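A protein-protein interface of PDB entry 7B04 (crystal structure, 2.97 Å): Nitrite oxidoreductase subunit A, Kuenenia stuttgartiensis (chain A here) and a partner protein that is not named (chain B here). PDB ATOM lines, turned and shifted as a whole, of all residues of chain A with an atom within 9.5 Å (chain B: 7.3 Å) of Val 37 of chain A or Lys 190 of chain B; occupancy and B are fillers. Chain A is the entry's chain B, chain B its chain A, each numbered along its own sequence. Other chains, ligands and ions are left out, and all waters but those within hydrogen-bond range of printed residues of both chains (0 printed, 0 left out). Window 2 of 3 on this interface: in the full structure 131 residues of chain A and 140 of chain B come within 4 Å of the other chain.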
ATOM      1  N   LYS A  32      10.702  13.639  12.006  1.00  0.00           N
ATOM      2  CA  LYS A  32      12.010  13.516  11.386  1.00  0.00           C
ATOM      3  C   LYS A  32      13.005  13.957  12.449  1.00  0.00           C
ATOM      4  O   LYS A  32      13.144  15.168  12.689  1.00  0.00           O
ATOM      5  CB  LYS A  32      12.098  14.378  10.134  1.00  0.00           C
ATOM      6  CG  LYS A  32      13.482  14.571   9.534  1.00  0.00           C
ATOM      7  CD  LYS A  32      13.360  15.355   8.222  1.00  0.00           C
ATOM      8  CE  LYS A  32      14.707  15.825   7.676  1.00  0.00           C
ATOM      9  NZ  LYS A  32      15.111  15.164   6.397  1.00  0.00           N
ATOM     10  N   ALA A  34      16.267  13.951  12.564  1.00  0.00           N
ATOM     11  CA  ALA A  34      17.484  14.575  12.082  1.00  0.00           C
ATOM     12  C   ALA A  34      17.349  14.862  10.594  1.00  0.00           C
ATOM     13  O   ALA A  34      16.594  14.197   9.879  1.00  0.00           O
ATOM     14  CB  ALA A  34      18.677  13.676  12.377  1.00  0.00           C
ATOM     15  N   VAL A  35      18.073  15.877  10.135  1.00  0.00           N
ATOM     16  CA  VAL A  35      18.061  16.286   8.735  1.00  0.00           C
ATOM     17  C   VAL A  35      19.224  15.624   8.010  1.00  0.00           C
ATOM     18  O   VAL A  35      20.382  15.743   8.431  1.00  0.00           O
ATOM     19  CB  VAL A  35      18.116  17.814   8.600  1.00  0.00           C
ATOM     20  CG1 VAL A  35      18.179  18.200   7.140  1.00  0.00           C
ATOM     21  CG2 VAL A  35      16.904  18.438   9.275  1.00  0.00           C
ATOM     22  N   VAL A  36      18.915  14.943   6.912  1.00  0.00           N
ATOM     23  CA  VAL A  36      19.892  14.202   6.126  1.00  0.00           C
ATOM     24  C   VAL A  36      20.092  14.912   4.795  1.00  0.00           C
ATOM     25  O   VAL A  36      19.120  15.299   4.132  1.00  0.00           O
ATOM     26  CB  VAL A  36      19.424  12.757   5.884  1.00  0.00           C
ATOM     27  CG1 VAL A  36      20.481  11.964   5.141  1.00  0.00           C
ATOM     28  CG2 VAL A  36      19.033  12.091   7.212  1.00  0.00           C
ATOM     29  N   VAL A  37      21.355  15.104   4.413  1.00  0.00           N
ATOM     30  CA  VAL A  37      21.729  15.717   3.145  1.00  0.00           C
ATOM     31  C   VAL A  37      22.537  14.688   2.362  1.00  0.00           C
ATOM     32  O   VAL A  37      23.445  14.051   2.917  1.00  0.00           O
ATOM     33  CB  VAL A  37      22.540  17.008   3.351  1.00  0.00           C
ATOM     34  CG1 VAL A  37      22.754  17.708   2.024  1.00  0.00           C
ATOM     35  CG2 VAL A  37      21.839  17.928   4.344  1.00  0.00           C
ATOM     36  N   ASP A  38      22.224  14.529   1.073  1.00  0.00           N
ATOM     37  CA  ASP A  38      22.869  13.479   0.268  1.00  0.00           C
ATOM     38  C   ASP A  38      24.086  14.012  -0.484  1.00  0.00           C
ATOM     39  O   ASP A  38      25.223  13.625  -0.198  1.00  0.00           O
ATOM     40  CB  ASP A  38      21.858  12.867  -0.704  1.00  0.00           C
ATOM     41  CG  ASP A  38      20.786  12.064  -0.001  1.00  0.00           C
ATOM     42  OD1 ASP A  38      21.073  11.517   1.082  1.00  0.00           O
ATOM     43  OD2 ASP A  38      19.661  11.971  -0.538  1.00  0.00           O
ATOM     44  N   ASN A  39      23.859  14.924  -1.424  1.00  0.00           N
ATOM     45  CA  ASN A  39      24.932  15.500  -2.226  1.00  0.00           C
ATOM     46  C   ASN A  39      24.674  16.990  -2.372  1.00  0.00           C
ATOM     47  O   ASN A  39      23.748  17.396  -3.085  1.00  0.00           O
ATOM     48  CB  ASN A  39      25.054  14.839  -3.603  1.00  0.00           C
ATOM     49  CG  ASN A  39      26.205  15.412  -4.424  1.00  0.00           C
ATOM     50  OD1 ASN A  39      26.930  16.297  -3.966  1.00  0.00           O
ATOM     51  ND2 ASN A  39      26.373  14.912  -5.641  1.00  0.00           N
ATOM     52  N   PRO A  40      25.458  17.827  -1.698  1.00  0.00           N
ATOM     53  CA  PRO A  40      25.227  19.277  -1.776  1.00  0.00           C
ATOM     54  C   PRO A  40      25.320  19.837  -3.186  1.00  0.00           C
ATOM     55  O   PRO A  40      24.655  20.836  -3.486  1.00  0.00           O
ATOM     56  CB  PRO A  40      26.323  19.844  -0.862  1.00  0.00           C
ATOM     57  CG  PRO A  40      26.707  18.702   0.037  1.00  0.00           C
ATOM     58  CD  PRO A  40      26.595  17.493  -0.825  1.00  0.00           C
ATOM     59  N   LEU A  41      26.125  19.228  -4.062  1.00  0.00           N
ATOM     60  CA  LEU A  41      26.165  19.664  -5.456  1.00  0.00           C
ATOM     61  C   LEU A  41      24.827  19.449  -6.153  1.00  0.00           C
ATOM     62  O   LEU A  41      24.421  20.262  -6.991  1.00  0.00           O
ATOM     63  CB  LEU A  41      27.268  18.928  -6.216  1.00  0.00           C
ATOM     64  CG  LEU A  41      28.724  19.222  -5.864  1.00  0.00           C
ATOM     65  CD1 LEU A  41      29.645  18.420  -6.771  1.00  0.00           C
ATOM     66  CD2 LEU A  41      29.017  20.711  -5.970  1.00  0.00           C
ATOM     67  N   ASP A  42      24.130  18.366  -5.820  1.00  0.00           N
ATOM     68  CA  ASP A  42      22.938  17.970  -6.563  1.00  0.00           C
ATOM     69  C   ASP A  42      21.662  18.521  -5.935  1.00  0.00           C
ATOM     70  O   ASP A  42      20.879  19.207  -6.602  1.00  0.00           O
ATOM     71  CB  ASP A  42      22.866  16.440  -6.653  1.00  0.00           C
ATOM     72  CG  ASP A  42      21.713  15.950  -7.518  1.00  0.00           C
ATOM     73  OD1 ASP A  42      21.014  16.785  -8.137  1.00  0.00           O
ATOM     74  OD2 ASP A  42      21.500  14.723  -7.574  1.00  0.00           O
ATOM     75  N   THR A  43      21.449  18.248  -4.651  1.00  0.00           N
ATOM     76  CA  THR A  43      20.155  18.515  -4.053  1.00  0.00           C
ATOM     77  C   THR A  43      20.337  18.879  -2.590  1.00  0.00           C
ATOM     78  O   THR A  43      21.313  18.477  -1.948  1.00  0.00           O
ATOM     79  CB  THR A  43      19.231  17.294  -4.198  1.00  0.00           C
ATOM     80  OG1 THR A  43      17.869  17.689  -3.991  1.00  0.00           O
ATOM     81  CG2 THR A  43      19.608  16.207  -3.200  1.00  0.00           C
ATOM     82  N   TYR A  44      19.400  19.673  -2.078  1.00  0.00           N
ATOM     83  CA  TYR A  44      19.419  20.105  -0.695  1.00  0.00           C
ATOM     84  C   TYR A  44      18.029  19.913  -0.107  1.00  0.00           C
ATOM     85  O   TYR A  44      17.027  20.232  -0.761  1.00  0.00           O
ATOM     86  CB  TYR A  44      19.856  21.571  -0.554  1.00  0.00           C
ATOM     87  CG  TYR A  44      20.327  21.923   0.842  1.00  0.00           C
ATOM     88  CD1 TYR A  44      21.509  21.395   1.349  1.00  0.00           C
ATOM     89  CD2 TYR A  44      19.591  22.776   1.654  1.00  0.00           C
ATOM     90  CE1 TYR A  44      21.947  21.708   2.625  1.00  0.00           C
ATOM     91  CE2 TYR A  44      20.023  23.095   2.933  1.00  0.00           C
ATOM     92  CZ  TYR A  44      21.200  22.558   3.413  1.00  0.00           C
ATOM     93  OH  TYR A  44      21.628  22.875   4.682  1.00  0.00           O
ATOM     94  N   PRO A  45      17.935  19.395   1.116  1.00  0.00           N
ATOM     95  CA  PRO A  45      16.627  19.018   1.651  1.00  0.00           C
ATOM     96  C   PRO A  45      15.717  20.205   1.862  1.00  0.00           C
ATOM     97  O   PRO A  45      14.547  20.166   1.475  1.00  0.00           O
ATOM     98  CB  PRO A  45      16.972  18.345   2.987  1.00  0.00           C
ATOM     99  CG  PRO A  45      18.390  17.934   2.841  1.00  0.00           C
ATOM    100  CD  PRO A  45      19.028  18.993   2.010  1.00  0.00           C
ATOM    101  N   ASP A  46      16.210  21.217   2.555  1.00  0.00           N
ATOM    102  CA  ASP A  46      15.327  22.357   2.899  1.00  0.00           C
ATOM    103  C   ASP A  46      16.019  23.686   2.609  1.00  0.00           C
ATOM    104  O   ASP A  46      17.093  23.887   3.122  1.00  0.00           O
ATOM    105  CB  ASP A  46      14.939  22.206   4.364  1.00  0.00           C
ATOM    106  CG  ASP A  46      13.944  23.201   4.871  1.00  0.00           C
ATOM    107  OD1 ASP A  46      13.436  23.907   4.074  1.00  0.00           O
ATOM    108  OD2 ASP A  46      13.717  23.233   6.054  1.00  0.00           O
ATOM    109  N   TRP A  49      15.255  28.678   4.517  1.00  0.00           N
ATOM    110  CA  TRP A  49      16.061  29.698   5.180  1.00  0.00           C
ATOM    111  C   TRP A  49      16.459  30.833   4.245  1.00  0.00           C
ATOM    112  O   TRP A  49      16.759  31.932   4.720  1.00  0.00           O
ATOM    113  CB  TRP A  49      17.325  29.074   5.773  1.00  0.00           C
ATOM    114  CG  TRP A  49      18.351  28.742   4.729  1.00  0.00           C
ATOM    115  CD1 TRP A  49      18.479  27.566   4.050  1.00  0.00           C
ATOM    116  CD2 TRP A  49      19.380  29.607   4.230  1.00  0.00           C
ATOM    117  NE1 TRP A  49      19.528  27.641   3.166  1.00  0.00           N
ATOM    118  CE2 TRP A  49      20.096  28.884   3.256  1.00  0.00           C
ATOM    119  CE3 TRP A  49      19.766  30.920   4.515  1.00  0.00           C
ATOM    120  CZ2 TRP A  49      21.177  29.431   2.566  1.00  0.00           C
ATOM    121  CZ3 TRP A  49      20.836  31.462   3.829  1.00  0.00           C
ATOM    122  CH2 TRP A  49      21.529  30.718   2.866  1.00  0.00           C
ATOM    123  N   TYR B  17      32.061  14.291  -4.036  1.00  0.00           N
ATOM    124  CA  TYR B  17      30.700  14.102  -4.524  1.00  0.00           C
ATOM    125  C   TYR B  17      30.697  13.916  -6.037  1.00  0.00           C
ATOM    126  O   TYR B  17      31.581  14.417  -6.744  1.00  0.00           O
ATOM    127  CB  TYR B  17      29.815  15.290  -4.142  1.00  0.00           C
ATOM    128  CG  TYR B  17      29.854  15.589  -2.661  1.00  0.00           C
ATOM    129  CD1 TYR B  17      29.099  14.843  -1.764  1.00  0.00           C
ATOM    130  CD2 TYR B  17      30.662  16.598  -2.154  1.00  0.00           C
ATOM    131  CE1 TYR B  17      29.138  15.107  -0.405  1.00  0.00           C
ATOM    132  CE2 TYR B  17      30.704  16.864  -0.795  1.00  0.00           C
ATOM    133  CZ  TYR B  17      29.939  16.116   0.073  1.00  0.00           C
ATOM    134  OH  TYR B  17      29.982  16.382   1.422  1.00  0.00           O
ATOM    135  N   LEU B 184      32.288  23.544   0.029  1.00  0.00           N
ATOM    136  CA  LEU B 184      31.194  22.576   0.046  1.00  0.00           C
ATOM    137  C   LEU B 184      31.685  21.190   0.440  1.00  0.00           C
ATOM    138  O   LEU B 184      31.042  20.499   1.241  1.00  0.00           O
ATOM    139  CB  LEU B 184      30.523  22.540  -1.326  1.00  0.00           C
ATOM    140  CG  LEU B 184      29.298  21.658  -1.559  1.00  0.00           C
ATOM    141  CD1 LEU B 184      28.323  22.367  -2.485  1.00  0.00           C
ATOM    142  CD2 LEU B 184      29.701  20.310  -2.140  1.00  0.00           C
ATOM    143  N   ALA B 186      34.289  20.620   2.207  1.00  0.00           N
ATOM    144  CA  ALA B 186      34.876  20.671   3.542  1.00  0.00           C
ATOM    145  C   ALA B 186      33.833  20.447   4.628  1.00  0.00           C
ATOM    146  O   ALA B 186      34.086  19.716   5.591  1.00  0.00           O
ATOM    147  CB  ALA B 186      35.584  22.008   3.751  1.00  0.00           C
ATOM    148  N   CYS B 187      32.664  21.066   4.496  1.00  0.00           N
ATOM    149  CA  CYS B 187      31.666  21.043   5.561  1.00  0.00           C
ATOM    150  C   CYS B 187      31.191  19.622   5.847  1.00  0.00           C
ATOM    151  O   CYS B 187      30.573  18.994   4.974  1.00  0.00           O
ATOM    152  CB  CYS B 187      30.474  21.925   5.204  1.00  0.00           C
ATOM    153  SG  CYS B 187      29.281  22.112   6.554  1.00  0.00           S
ATOM    154  N   PRO B 188      31.451  19.083   7.043  1.00  0.00           N
ATOM    155  CA  PRO B 188      30.985  17.730   7.375  1.00  0.00           C
ATOM    156  C   PRO B 188      29.487  17.634   7.623  1.00  0.00           C
ATOM    157  O   PRO B 188      28.962  16.514   7.682  1.00  0.00           O
ATOM    158  CB  PRO B 188      31.777  17.390   8.650  1.00  0.00           C
ATOM    159  CG  PRO B 188      32.897  18.400   8.694  1.00  0.00           C
ATOM    160  CD  PRO B 188      32.302  19.634   8.107  1.00  0.00           C
ATOM    161  N   ARG B 189      28.794  18.754   7.817  1.00  0.00           N
ATOM    162  CA  ARG B 189      27.345  18.744   7.965  1.00  0.00           C
ATOM    163  C   ARG B 189      26.623  18.866   6.636  1.00  0.00           C
ATOM    164  O   ARG B 189      25.389  18.801   6.613  1.00  0.00           O
ATOM    165  CB  ARG B 189      26.879  19.896   8.856  1.00  0.00           C
ATOM    166  CG  ARG B 189      27.698  20.135  10.085  1.00  0.00           C
ATOM    167  CD  ARG B 189      27.235  21.406  10.798  1.00  0.00           C
ATOM    168  NE  ARG B 189      25.788  21.606  10.734  1.00  0.00           N
ATOM    169  CZ  ARG B 189      24.884  20.817  11.310  1.00  0.00           C
ATOM    170  NH1 ARG B 189      25.261  19.752  12.005  1.00  0.00           N
ATOM    171  NH2 ARG B 189      23.594  21.094  11.184  1.00  0.00           N
ATOM    172  N   LYS B 190      27.359  19.032   5.537  1.00  0.00           N
ATOM    173  CA  LYS B 190      26.770  19.323   4.234  1.00  0.00           C
ATOM    174  C   LYS B 190      25.823  20.517   4.332  1.00  0.00           C
ATOM    175  O   LYS B 190      24.727  20.522   3.769  1.00  0.00           O
ATOM    176  CB  LYS B 190      26.063  18.091   3.665  1.00  0.00           C
ATOM    177  CG  LYS B 190      26.919  16.832   3.716  1.00  0.00           C
ATOM    178  CD  LYS B 190      26.323  15.703   2.892  1.00  0.00           C
ATOM    179  CE  LYS B 190      27.131  14.425   3.060  1.00  0.00           C
ATOM    180  NZ  LYS B 190      26.760  13.392   2.054  1.00  0.00           N
ATOM    181  N   ALA B 191      26.254  21.538   5.075  1.00  0.00           N
ATOM    182  CA  ALA B 191      25.489  22.768   5.235  1.00  0.00           C
ATOM    183  C   ALA B 191      25.744  23.777   4.124  1.00  0.00           C
ATOM    184  O   ALA B 191      25.011  24.766   4.026  1.00  0.00           O
ATOM    185  CB  ALA B 191      25.803  23.412   6.590  1.00  0.00           C
ATOM    186  N   ILE B 192      26.763  23.560   3.299  1.00  0.00           N
ATOM    187  CA  ILE B 192      27.001  24.357   2.103  1.00  0.00           C
ATOM    188  C   ILE B 192      26.497  23.560   0.911  1.00  0.00           C
ATOM    189  O   ILE B 192      26.846  22.383   0.756  1.00  0.00           O
ATOM    190  CB  ILE B 192      28.490  24.707   1.945  1.00  0.00           C
ATOM    191  CG1 ILE B 192      29.029  25.321   3.237  1.00  0.00           C
ATOM    192  CG2 ILE B 192      28.689  25.649   0.771  1.00  0.00           C
ATOM    193  CD1 ILE B 192      30.289  26.140   3.052  1.00  0.00           C
ATOM    194  N   TYR B 193      25.686  24.190   0.066  1.00  0.00           N
ATOM    195  CA  TYR B 193      25.082  23.498  -1.062  1.00  0.00           C
ATOM    196  C   TYR B 193      25.122  24.385  -2.296  1.00  0.00           C
ATOM    197  O   TYR B 193      25.089  25.614  -2.202  1.00  0.00           O
ATOM    198  CB  TYR B 193      23.636  23.079  -0.760  1.00  0.00           C
ATOM    199  CG  TYR B 193      22.682  24.231  -0.529  1.00  0.00           C
ATOM    200  CD1 TYR B 193      22.575  24.830   0.719  1.00  0.00           C
ATOM    201  CD2 TYR B 193      21.878  24.710  -1.557  1.00  0.00           C
ATOM    202  CE1 TYR B 193      21.701  25.879   0.936  1.00  0.00           C
ATOM    203  CE2 TYR B 193      21.001  25.759  -1.350  1.00  0.00           C
ATOM    204  CZ  TYR B 193      20.917  26.339  -0.100  1.00  0.00           C
ATOM    205  OH  TYR B 193      20.047  27.383   0.113  1.00  0.00           O
ATOM    206  N   LEU B 202      25.897  28.474  -1.369  1.00  0.00           N
ATOM    207  CA  LEU B 202      25.362  29.166  -0.207  1.00  0.00           C
ATOM    208  C   LEU B 202      25.664  28.384   1.062  1.00  0.00           C
ATOM    209  O   LEU B 202      25.783  27.156   1.042  1.00  0.00           O
ATOM    210  CB  LEU B 202      23.848  29.371  -0.329  1.00  0.00           C
ATOM    211  CG  LEU B 202      23.382  30.507  -1.236  1.00  0.00           C
ATOM    212  CD1 LEU B 202      21.992  30.219  -1.777  1.00  0.00           C
ATOM    213  CD2 LEU B 202      23.401  31.817  -0.477  1.00  0.00           C
ATOM    214  N   ASP B 204      24.018  27.447   4.567  1.00  0.00           N
ATOM    215  CA  ASP B 204      22.744  27.406   5.280  1.00  0.00           C
ATOM    216  C   ASP B 204      22.940  28.027   6.656  1.00  0.00           C
ATOM    217  O   ASP B 204      23.588  27.435   7.526  1.00  0.00           O
ATOM    218  CB  ASP B 204      22.236  25.969   5.383  1.00  0.00           C
ATOM    219  CG  ASP B 204      20.914  25.848   6.155  1.00  0.00           C
ATOM    220  OD1 ASP B 204      20.219  24.828   5.964  1.00  0.00           O
ATOM    221  OD2 ASP B 204      20.559  26.743   6.951  1.00  0.00           O
ATOM    222  N   ARG B 207      21.508  25.931   9.613  1.00  0.00           N
ATOM    223  CA  ARG B 207      22.144  24.671   9.970  1.00  0.00           C
ATOM    224  C   ARG B 207      23.643  24.771  10.203  1.00  0.00           C
ATOM    225  O   ARG B 207      24.224  23.830  10.750  1.00  0.00           O
ATOM    226  CB  ARG B 207      21.905  23.622   8.873  1.00  0.00           C
ATOM    227  CG  ARG B 207      20.484  23.110   8.769  1.00  0.00           C
ATOM    228  CD  ARG B 207      20.389  22.001   7.733  1.00  0.00           C
ATOM    229  NE  ARG B 207      21.118  20.804   8.143  1.00  0.00           N
ATOM    230  CZ  ARG B 207      22.262  20.400   7.601  1.00  0.00           C
ATOM    231  NH1 ARG B 207      22.852  19.297   8.041  1.00  0.00           N
ATOM    232  NH2 ARG B 207      22.818  21.098   6.620  1.00  0.00           N
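The side-chain amino group of Lys 190 of chain B lies close to the backbone carbonyl oxygen of Val 37 of chain A (3.5 Å). The backbone carbonyl oxygen of Asp 38 of chain A sits at hydrogen-bond distance from the side-chain amino group of Lys 190 of chain B (2.7 Å). The indole nitrogen (NE1) of Trp 49 of chain A sits at hydrogen-bond distance from the side-chain hydroxyl (OH) of Tyr 193 of chain B (3.1 Å). The side-chain carboxylate (OD1) of Asp 204 of chain B lies within hydrogen-bond range of the side-chain hydroxyl (OH) of Tyr 44 of chain A (2.7 Å). The side-chain hydroxyl (OH) of Tyr 44 of chain A sits at hydrogen-bond distance from the guanidinium group (NH2) of Arg 207 of chain B (2.9 Å).
Printed residues of chain A that touch a printed residue of chain B: Val 37, Asp 38, Asn 39, Pro 40, Leu 41, Tyr 44 and Trp 49. Hydrophobic or aromatic side chains of chain A that line the printed part of chain B: Val 37, Pro 40, Leu 41, Tyr 44 and Trp 49. Of the 13 printed residues of chain B, 9 touch a printed residue of chain A. Among the printed residues, 17 pairs touch across the chains.
Among the printed residues, pairs that only touch across the chains: Pro 40 of chain A with Ile 192 of chain B, Asn 39 of chain A with Tyr 17 of chain B, Tyr 44 of chain A with Lys 190 of chain B, Tyr 44 of chain A with Tyr 193 of chain B, Pro 40 of chain A with Tyr 17 of chain B, Pro 40 of chain A with Leu 184 of chain B, Pro 40 of chain A with Tyr 193 of chain B, Trp 49 of chain A with Asp 204 of chain B, Pro 40 of chain A with Lys 190 of chain B, Tyr 44 of chain A with Ala 191 of chain B, Leu 41 of chain A with Leu 184 of chain B and Trp 49 of chain A with Leu 202 of chain B.
The backbone NH (N) of Ala 191 of chain B sits close to the side-chain sulfur (SG) of Cys 187 of chain B, 3.4 Å away. The backbone carbonyl oxygen (O) of Arg 207 of chain B is in hydrogen-bond range of the guanidinium group (NE) of Arg 189 of chain B, 2.7 Å away. The guanidinium group (NH2) of Arg 207 of chain B is in hydrogen-bond range of the backbone carbonyl oxygen (O) of Lys 190 of chain B, 3.5 Å away. O of Ala 191 of chain B is in hydrogen-bond range of N of Asp 204 of chain B. The side-chain carboxylate of Asp 204 of chain B lies within hydrogen-bond range of the backbone NH of Arg 207 of chain B. The backbone NH of Leu 41 of chain A sits at hydrogen-bond distance from the side-chain amide oxygen of Asn 39 of chain A (3.0 Å).
Val 37 of chain A touches one residue of chain B. Lys 190 of chain B touches just these residues of chain A: Val 37, Asp 38, Pro 40 and Tyr 44. Of the printed residues of chain A, Ala 191 of chain B touches Tyr 44 (3.9 Å). Printed residues of chain A within 4 Å of Asp 204 of chain B: Tyr 44 (2.7 Å) and Trp 49 (3.6 Å). Printed residues of chain A within 4 Å of Leu 184 of chain B: Pro 40 and Leu 41. Asp 46 of chain A touches none of the printed residues of chain B. The nearest printed residue of chain A that does not touch Tyr 193 of chain B is Thr 43 of chain A (5.3 Å).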
